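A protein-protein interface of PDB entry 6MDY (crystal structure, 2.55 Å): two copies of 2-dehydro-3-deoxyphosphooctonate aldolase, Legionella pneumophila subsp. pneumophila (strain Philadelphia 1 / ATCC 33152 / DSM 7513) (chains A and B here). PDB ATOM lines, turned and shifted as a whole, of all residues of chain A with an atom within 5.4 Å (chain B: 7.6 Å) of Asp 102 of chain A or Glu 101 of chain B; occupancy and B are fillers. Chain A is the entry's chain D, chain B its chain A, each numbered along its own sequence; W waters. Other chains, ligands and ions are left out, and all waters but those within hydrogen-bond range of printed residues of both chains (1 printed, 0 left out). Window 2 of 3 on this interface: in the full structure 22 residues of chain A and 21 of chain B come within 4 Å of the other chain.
Of the printed residues of chain B, Glu 101 of chain A touches His 100, Glu 101 and Asp 102.
Of the printed residues of chain B, Asp 102 of chain A touches Glu 101.
Of the printed residues of chain A, Glu 101 of chain B touches His 100, Glu 101 and Asp 102.
Of the printed residues of chain A, Asp 102 of chain B touches Glu 101 (3.8 Å).
Pro 118 of chain B touches none of the printed residues of chain A.
Lys 130 of chain B touches none of the printed residues of chain A.
The nearest residue of chain B that does not touch Asp 102 of chain A is Asp 102 of chain B (4.8 Å).
The nearest printed residue of chain B that does not touch Arg 66 of chain A is Glu 101 of chain B (4.9 Å).
Water W1 lies within hydrogen-bond range of N of Phe 127 of chain B (3.1 Å), ND2 of Asn 126 of chain B (3.2 Å) and O of Arg 66 of chain A (3.5 Å).
His 100 of chain A touches Glu 101 of chain B, and with the chains exchanged Glu 101 of chain A touches His 100 of chain B.
Glu 101 of chain B touches its own counterpart, Glu 101 of chain A.
Glu 101 of chain A touches Asp 102 of chain B, and with the chains exchanged Asp 102 of chain A touches Glu 101 of chain B.
Phe 120 of chain A touches Leu 121 of chain B, and with the chains exchanged Leu 121 of chain A touches Phe 120 of chain B.
7 positions are printed for both chains.
Of the 13 pairs that touch across the chains among the printed residues, 8 have their exchanged pair printed and touching as well.
Among the printed residues, merely in contact across the chains: Phe 120 of chain A with Gln 124 of chain B (3.4 Å), Phe 120 of chain A with Phe 120 of chain B (3.4 Å), Arg 66 of chain A with Asn 126 of chain B (3.6 Å), Glu 101 of chain A with His 100 of chain B (3.6 Å), Phe 120 of chain A with Leu 121 of chain B (3.7 Å), Glu 101 of chain A with Glu 101 of chain B (3.7 Å), His 100 of chain A with Glu 101 of chain B (3.7 Å), Glu 101 of chain A with Asp 102 of chain B (3.8 Å), Asp 102 of chain A with Glu 101 of chain B (3.9 Å), His 100 of chain A with Gln 124 of chain B (3.9 Å) and Leu 121 of chain A with Phe 120 of chain B (3.95 Å).
N of His 100 of chain B lies within hydrogen-bond range of OG1 of Thr 103 of chain B, at 2.4 Å.
The side-chain amino group (NZ) of Lys 130 of chain B is in hydrogen-bond range of the side-chain amide oxygen (OD1) of Asn 126 of chain B, 2.8 Å away.
OD1 of Asp 102 of chain A is in salt-bridge range of NH2 of Arg 66 of chain A (2.7 Å).
N of His 100 of chain A sits at hydrogen-bond distance from OG1 of Thr 103 of chain A, 2.7 Å away.
The backbone NH (N) of Arg 66 of chain A sits at hydrogen-bond distance from the side-chain amide oxygen (OE1) of Gln 124 of chain B (3.1 Å).
The backbone NH (N) of Thr 125 of chain B is in hydrogen-bond range of the backbone carbonyl oxygen (O) of Arg 66 of chain A (3.3 Å).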
ATOM      1  N   ARG A  66      10.505  34.534 -21.290  1.00  0.00           N
ATOM      2  CA  ARG A  66       9.179  34.184 -21.780  1.00  0.00           C
ATOM      3  C   ARG A  66       8.105  34.555 -20.763  1.00  0.00           C
ATOM      4  O   ARG A  66       8.283  34.386 -19.552  1.00  0.00           O
ATOM      5  CB  ARG A  66       9.115  32.690 -22.105  1.00  0.00           C
ATOM      6  CG  ARG A  66      10.001  32.258 -23.269  1.00  0.00           C
ATOM      7  CD  ARG A  66       9.283  31.232 -24.128  1.00  0.00           C
ATOM      8  NE  ARG A  66       9.884  29.904 -24.029  1.00  0.00           N
ATOM      9  CZ  ARG A  66       9.243  28.772 -24.306  1.00  0.00           C
ATOM     10  NH1 ARG A  66       7.973  28.799 -24.690  1.00  0.00           N
ATOM     11  NH2 ARG A  66       9.870  27.609 -24.192  1.00  0.00           N
ATOM     12  N   HIS A 100      15.019  27.594 -26.124  1.00  0.00           N
ATOM     13  CA  HIS A 100      15.009  27.386 -24.683  1.00  0.00           C
ATOM     14  C   HIS A 100      15.163  25.898 -24.403  1.00  0.00           C
ATOM     15  O   HIS A 100      15.225  25.074 -25.320  1.00  0.00           O
ATOM     16  CB  HIS A 100      13.730  27.942 -24.054  1.00  0.00           C
ATOM     17  CG  HIS A 100      13.699  29.436 -23.943  1.00  0.00           C
ATOM     18  ND1 HIS A 100      14.295  30.271 -24.865  1.00  0.00           N
ATOM     19  CD2 HIS A 100      13.123  30.243 -23.021  1.00  0.00           C
ATOM     20  CE1 HIS A 100      14.093  31.529 -24.511  1.00  0.00           C
ATOM     21  NE2 HIS A 100      13.382  31.538 -23.398  1.00  0.00           N
ATOM     22  N   GLU A 101      15.202  25.546 -23.117  1.00  0.00           N
ATOM     23  CA  GLU A 101      15.395  24.147 -22.752  1.00  0.00           C
ATOM     24  C   GLU A 101      14.249  23.263 -23.234  1.00  0.00           C
ATOM     25  O   GLU A 101      14.439  22.051 -23.378  1.00  0.00           O
ATOM     26  CB  GLU A 101      15.587  24.011 -21.241  1.00  0.00           C
ATOM     27  CG  GLU A 101      16.887  24.622 -20.730  1.00  0.00           C
ATOM     28  CD  GLU A 101      17.079  24.442 -19.230  1.00  0.00           C
ATOM     29  OE1 GLU A 101      18.080  23.798 -18.833  1.00  0.00           O
ATOM     30  OE2 GLU A 101      16.227  24.940 -18.453  1.00  0.00           O
ATOM     31  N   ASP A 102      13.066  23.822 -23.477  1.00  0.00           N
ATOM     32  CA  ASP A 102      11.929  23.026 -23.925  1.00  0.00           C
ATOM     33  C   ASP A 102      11.579  23.248 -25.395  1.00  0.00           C
ATOM     34  O   ASP A 102      10.544  22.761 -25.852  1.00  0.00           O
ATOM     35  CB  ASP A 102      10.712  23.320 -23.046  1.00  0.00           C
ATOM     36  CG  ASP A 102      10.390  24.803 -22.980  1.00  0.00           C
ATOM     37  OD1 ASP A 102      11.329  25.630 -23.132  1.00  0.00           O
ATOM     38  OD2 ASP A 102       9.200  25.135 -22.781  1.00  0.00           O
ATOM     39  N   THR A 103      12.406  23.951 -26.139  1.00  0.00           N
ATOM     40  CA  THR A 103      12.147  24.154 -27.558  1.00  0.00           C
ATOM     41  C   THR A 103      12.475  22.887 -28.351  1.00  0.00           C
ATOM     42  O   THR A 103      13.495  22.241 -28.098  1.00  0.00           O
ATOM     43  CB  THR A 103      12.971  25.324 -28.104  1.00  0.00           C
ATOM     44  OG1 THR A 103      12.841  26.454 -27.230  1.00  0.00           O
ATOM     45  CG2 THR A 103      12.476  25.717 -29.486  1.00  0.00           C
ATOM     46  N   PRO A 104      11.620  22.498 -29.303  1.00  0.00           N
ATOM     47  CA  PRO A 104      12.006  21.422 -30.229  1.00  0.00           C
ATOM     48  C   PRO A 104      13.096  21.886 -31.182  1.00  0.00           C
ATOM     49  O   PRO A 104      12.821  22.628 -32.130  1.00  0.00           O
ATOM     50  CB  PRO A 104      10.702  21.098 -30.973  1.00  0.00           C
ATOM     51  CG  PRO A 104       9.849  22.315 -30.818  1.00  0.00           C
ATOM     52  CD  PRO A 104      10.237  22.959 -29.512  1.00  0.00           C
ATOM     53  N   PHE A 120      20.349  33.885 -19.895  1.00  0.00           N
ATOM     54  CA  PHE A 120      20.092  33.205 -18.633  1.00  0.00           C
ATOM     55  C   PHE A 120      20.358  31.703 -18.700  1.00  0.00           C
ATOM     56  O   PHE A 120      20.348  31.042 -17.654  1.00  0.00           O
ATOM     57  CB  PHE A 120      18.656  33.487 -18.166  1.00  0.00           C
ATOM     58  CG  PHE A 120      17.596  32.746 -18.935  1.00  0.00           C
ATOM     59  CD1 PHE A 120      17.077  33.269 -20.109  1.00  0.00           C
ATOM     60  CD2 PHE A 120      17.095  31.538 -18.467  1.00  0.00           C
ATOM     61  CE1 PHE A 120      16.084  32.591 -20.820  1.00  0.00           C
ATOM     62  CE2 PHE A 120      16.101  30.854 -19.176  1.00  0.00           C
ATOM     63  CZ  PHE A 120      15.597  31.382 -20.352  1.00  0.00           C
ATOM     64  N   LEU A 121      20.629  31.153 -19.882  1.00  0.00           N
ATOM     65  CA  LEU A 121      20.907  29.732 -20.033  1.00  0.00           C
ATOM     66  C   LEU A 121      22.385  29.428 -20.260  1.00  0.00           C
ATOM     67  O   LEU A 121      22.735  28.256 -20.447  1.00  0.00           O
ATOM     68  CB  LEU A 121      20.080  29.154 -21.194  1.00  0.00           C
ATOM     69  CG  LEU A 121      18.567  29.015 -20.952  1.00  0.00           C
ATOM     70  CD1 LEU A 121      17.829  28.618 -22.230  1.00  0.00           C
ATOM     71  CD2 LEU A 121      18.252  28.032 -19.804  1.00  0.00           C
ATOM     72  N   VAL B  99      13.170  21.784 -10.370  1.00  0.00           N
ATOM     73  CA  VAL B  99      12.621  21.456 -11.673  1.00  0.00           C
ATOM     74  C   VAL B  99      13.100  22.532 -12.635  1.00  0.00           C
ATOM     75  O   VAL B  99      13.306  23.686 -12.245  1.00  0.00           O
ATOM     76  CB  VAL B  99      11.083  21.412 -11.586  1.00  0.00           C
ATOM     77  CG1 VAL B  99      10.661  20.322 -10.614  1.00  0.00           C
ATOM     78  CG2 VAL B  99      10.563  22.763 -11.076  1.00  0.00           C
ATOM     79  N   HIS B 100      13.295  22.144 -13.883  1.00  0.00           N
ATOM     80  CA  HIS B 100      13.721  23.022 -14.956  1.00  0.00           C
ATOM     81  C   HIS B 100      12.576  23.155 -15.950  1.00  0.00           C
ATOM     82  O   HIS B 100      11.496  22.579 -15.769  1.00  0.00           O
ATOM     83  CB  HIS B 100      14.972  22.467 -15.628  1.00  0.00           C
ATOM     84  CG  HIS B 100      16.228  22.653 -14.836  1.00  0.00           C
ATOM     85  ND1 HIS B 100      17.468  22.729 -15.433  1.00  0.00           N
ATOM     86  CD2 HIS B 100      16.444  22.771 -13.505  1.00  0.00           C
ATOM     87  CE1 HIS B 100      18.393  22.895 -14.507  1.00  0.00           C
ATOM     88  NE2 HIS B 100      17.799  22.924 -13.327  1.00  0.00           N
ATOM     89  N   GLU B 101      12.824  23.927 -17.009  1.00  0.00           N
ATOM     90  CA  GLU B 101      11.803  24.134 -18.029  1.00  0.00           C
ATOM     91  C   GLU B 101      11.419  22.834 -18.726  1.00  0.00           C
ATOM     92  O   GLU B 101      10.309  22.728 -19.254  1.00  0.00           O
ATOM     93  CB  GLU B 101      12.286  25.157 -19.057  1.00  0.00           C
ATOM     94  CG  GLU B 101      12.478  26.566 -18.502  1.00  0.00           C
ATOM     95  CD  GLU B 101      12.907  27.555 -19.576  1.00  0.00           C
ATOM     96  OE1 GLU B 101      14.004  27.369 -20.151  1.00  0.00           O
ATOM     97  OE2 GLU B 101      12.141  28.511 -19.850  1.00  0.00           O
ATOM     98  N   ASP B 102      12.305  21.841 -18.731  1.00  0.00           N
ATOM     99  CA  ASP B 102      12.045  20.560 -19.375  1.00  0.00           C
ATOM    100  C   ASP B 102      11.794  19.437 -18.371  1.00  0.00           C
ATOM    101  O   ASP B 102      11.810  18.262 -18.751  1.00  0.00           O
ATOM    102  CB  ASP B 102      13.203  20.194 -20.311  1.00  0.00           C
ATOM    103  CG  ASP B 102      14.546  20.135 -19.596  1.00  0.00           C
ATOM    104  OD1 ASP B 102      14.759  20.891 -18.613  1.00  0.00           O
ATOM    105  OD2 ASP B 102      15.392  19.321 -20.022  1.00  0.00           O
ATOM    106  N   THR B 103      11.588  19.767 -17.100  1.00  0.00           N
ATOM    107  CA  THR B 103      11.277  18.747 -16.106  1.00  0.00           C
ATOM    108  C   THR B 103       9.842  18.280 -16.298  1.00  0.00           C
ATOM    109  O   THR B 103       8.940  19.117 -16.417  1.00  0.00           O
ATOM    110  CB  THR B 103      11.438  19.303 -14.689  1.00  0.00           C
ATOM    111  OG1 THR B 103      12.756  19.842 -14.518  1.00  0.00           O
ATOM    112  CG2 THR B 103      11.175  18.218 -13.646  1.00  0.00           C
ATOM    113  N   PRO B 104       9.581  16.962 -16.327  1.00  0.00           N
ATOM    114  CA  PRO B 104       8.185  16.496 -16.318  1.00  0.00           C
ATOM    115  C   PRO B 104       7.566  16.719 -14.949  1.00  0.00           C
ATOM    116  O   PRO B 104       7.817  15.955 -14.010  1.00  0.00           O
ATOM    117  CB  PRO B 104       8.297  15.006 -16.669  1.00  0.00           C
ATOM    118  CG  PRO B 104       9.687  14.625 -16.300  1.00  0.00           C
ATOM    119  CD  PRO B 104      10.545  15.855 -16.434  1.00  0.00           C
ATOM    120  N   LEU B 105       6.738  17.760 -14.838  1.00  0.00           N
ATOM    121  CA  LEU B 105       6.279  18.206 -13.527  1.00  0.00           C
ATOM    122  C   LEU B 105       5.395  17.174 -12.839  1.00  0.00           C
ATOM    123  O   LEU B 105       5.560  16.924 -11.642  1.00  0.00           O
ATOM    124  CB  LEU B 105       5.543  19.538 -13.655  1.00  0.00           C
ATOM    125  CG  LEU B 105       6.396  20.737 -14.076  1.00  0.00           C
ATOM    126  CD1 LEU B 105       5.613  22.034 -13.892  1.00  0.00           C
ATOM    127  CD2 LEU B 105       7.712  20.773 -13.308  1.00  0.00           C
ATOM    128  N   PRO B 118      15.120  27.076  -9.761  1.00  0.00           N
ATOM    129  CA  PRO B 118      16.497  27.576  -9.645  1.00  0.00           C
ATOM    130  C   PRO B 118      16.591  29.063  -9.959  1.00  0.00           C
ATOM    131  O   PRO B 118      15.763  29.633 -10.675  1.00  0.00           O
ATOM    132  CB  PRO B 118      17.278  26.739 -10.666  1.00  0.00           C
ATOM    133  CG  PRO B 118      16.248  26.128 -11.558  1.00  0.00           C
ATOM    134  CD  PRO B 118      14.984  26.021 -10.780  1.00  0.00           C
ATOM    135  N   PHE B 120      18.420  30.904 -11.824  1.00  0.00           N
ATOM    136  CA  PHE B 120      18.567  31.406 -13.185  1.00  0.00           C
ATOM    137  C   PHE B 120      17.254  31.401 -13.963  1.00  0.00           C
ATOM    138  O   PHE B 120      17.214  31.958 -15.066  1.00  0.00           O
ATOM    139  CB  PHE B 120      19.643  30.596 -13.930  1.00  0.00           C
ATOM    140  CG  PHE B 120      19.216  29.202 -14.295  1.00  0.00           C
ATOM    141  CD1 PHE B 120      19.399  28.153 -13.405  1.00  0.00           C
ATOM    142  CD2 PHE B 120      18.631  28.935 -15.532  1.00  0.00           C
ATOM    143  CE1 PHE B 120      18.996  26.856 -13.737  1.00  0.00           C
ATOM    144  CE2 PHE B 120      18.236  27.647 -15.872  1.00  0.00           C
ATOM    145  CZ  PHE B 120      18.414  26.606 -14.968  1.00  0.00           C
ATOM    146  N   LEU B 121      16.186  30.814 -13.411  1.00  0.00           N
ATOM    147  CA  LEU B 121      14.877  30.753 -14.056  1.00  0.00           C
ATOM    148  C   LEU B 121      13.853  31.699 -13.448  1.00  0.00           C
ATOM    149  O   LEU B 121      12.688  31.667 -13.857  1.00  0.00           O
ATOM    150  CB  LEU B 121      14.327  29.324 -14.012  1.00  0.00           C
ATOM    151  CG  LEU B 121      15.030  28.348 -14.960  1.00  0.00           C
ATOM    152  CD1 LEU B 121      14.546  26.913 -14.780  1.00  0.00           C
ATOM    153  CD2 LEU B 121      14.883  28.800 -16.414  1.00  0.00           C
ATOM    154  N   GLN B 124      11.583  33.574 -15.770  1.00  0.00           N
ATOM    155  CA  GLN B 124      10.758  32.846 -16.742  1.00  0.00           C
ATOM    156  C   GLN B 124       9.351  32.665 -16.172  1.00  0.00           C
ATOM    157  O   GLN B 124       8.996  31.622 -15.621  1.00  0.00           O
ATOM    158  CB  GLN B 124      11.392  31.502 -17.094  1.00  0.00           C
ATOM    159  CG  GLN B 124      12.794  31.596 -17.635  1.00  0.00           C
ATOM    160  CD  GLN B 124      12.936  32.661 -18.703  1.00  0.00           C
ATOM    161  OE1 GLN B 124      12.339  32.567 -19.776  1.00  0.00           O
ATOM    162  NE2 GLN B 124      13.725  33.694 -18.410  1.00  0.00           N
ATOM    163  N   THR B 125       8.529  33.709 -16.328  1.00  0.00           N
ATOM    164  CA  THR B 125       7.214  33.737 -15.688  1.00  0.00           C
ATOM    165  C   THR B 125       6.360  32.560 -16.132  1.00  0.00           C
ATOM    166  O   THR B 125       5.718  31.899 -15.310  1.00  0.00           O
ATOM    167  CB  THR B 125       6.489  35.044 -16.006  1.00  0.00           C
ATOM    168  OG1 THR B 125       7.329  36.161 -15.698  1.00  0.00           O
ATOM    169  CG2 THR B 125       5.207  35.132 -15.209  1.00  0.00           C
ATOM    170  N   ASN B 126       6.325  32.303 -17.440  1.00  0.00           N
ATOM    171  CA  ASN B 126       5.562  31.182 -17.974  1.00  0.00           C
ATOM    172  C   ASN B 126       5.941  29.876 -17.286  1.00  0.00           C
ATOM    173  O   ASN B 126       5.072  29.059 -16.966  1.00  0.00           O
ATOM    174  CB  ASN B 126       5.783  31.104 -19.485  1.00  0.00           C
ATOM    175  CG  ASN B 126       5.549  29.722 -20.052  1.00  0.00           C
ATOM    176  OD1 ASN B 126       4.406  29.306 -20.249  1.00  0.00           O
ATOM    177  ND2 ASN B 126       6.638  29.011 -20.350  1.00  0.00           N
ATOM    178  N   PHE B 127       7.230  29.679 -17.015  1.00  0.00           N
ATOM    179  CA  PHE B 127       7.650  28.465 -16.329  1.00  0.00           C
ATOM    180  C   PHE B 127       7.285  28.499 -14.846  1.00  0.00           C
ATOM    181  O   PHE B 127       6.836  27.488 -14.294  1.00  0.00           O
ATOM    182  CB  PHE B 127       9.152  28.264 -16.517  1.00  0.00           C
ATOM    183  CG  PHE B 127       9.783  27.405 -15.470  1.00  0.00           C
ATOM    184  CD1 PHE B 127       9.718  26.024 -15.555  1.00  0.00           C
ATOM    185  CD2 PHE B 127      10.445  27.981 -14.393  1.00  0.00           C
ATOM    186  CE1 PHE B 127      10.304  25.226 -14.579  1.00  0.00           C
ATOM    187  CE2 PHE B 127      11.034  27.192 -13.420  1.00  0.00           C
ATOM    188  CZ  PHE B 127      10.963  25.811 -13.511  1.00  0.00           C
ATOM    189  N   ILE B 128       7.465  29.646 -14.182  1.00  0.00           N
ATOM    190  CA  ILE B 128       7.105  29.750 -12.767  1.00  0.00           C
ATOM    191  C   ILE B 128       5.631  29.412 -12.553  1.00  0.00           C
ATOM    192  O   ILE B 128       5.277  28.670 -11.629  1.00  0.00           O
ATOM    193  CB  ILE B 128       7.441  31.155 -12.225  1.00  0.00           C
ATOM    194  CG1 ILE B 128       8.932  31.477 -12.389  1.00  0.00           C
ATOM    195  CG2 ILE B 128       7.007  31.288 -10.768  1.00  0.00           C
ATOM    196  CD1 ILE B 128       9.872  30.642 -11.528  1.00  0.00           C
ATOM    197  N   LYS B 130       3.685  27.528 -14.409  1.00  0.00           N
ATOM    198  CA  LYS B 130       3.459  26.098 -14.602  1.00  0.00           C
ATOM    199  C   LYS B 130       3.836  25.315 -13.352  1.00  0.00           C
ATOM    200  O   LYS B 130       3.158  24.344 -12.992  1.00  0.00           O
ATOM    201  CB  LYS B 130       4.239  25.592 -15.819  1.00  0.00           C
ATOM    202  CG  LYS B 130       3.714  26.133 -17.133  1.00  0.00           C
ATOM    203  CD  LYS B 130       4.486  25.610 -18.331  1.00  0.00           C
ATOM    204  CE  LYS B 130       3.807  26.035 -19.628  1.00  0.00           C
ATOM    205  NZ  LYS B 130       4.776  26.521 -20.648  1.00  0.00           N
ATOM    206  N   VAL B 131       4.919  25.726 -12.683  1.00  0.00           N
ATOM    207  CA  VAL B 131       5.343  25.075 -11.445  1.00  0.00           C
ATOM    208  C   VAL B 131       4.315  25.304 -10.347  1.00  0.00           C
ATOM    209  O   VAL B 131       3.903  24.367  -9.650  1.00  0.00           O
ATOM    210  CB  VAL B 131       6.736  25.589 -11.027  1.00  0.00           C
ATOM    211  CG1 VAL B 131       7.122  25.051  -9.660  1.00  0.00           C
ATOM    212  CG2 VAL B 131       7.780  25.209 -12.068  1.00  0.00           C
HETATM  213  O   HOH W   1       8.858  30.994 -19.252  1.00  0.00           O
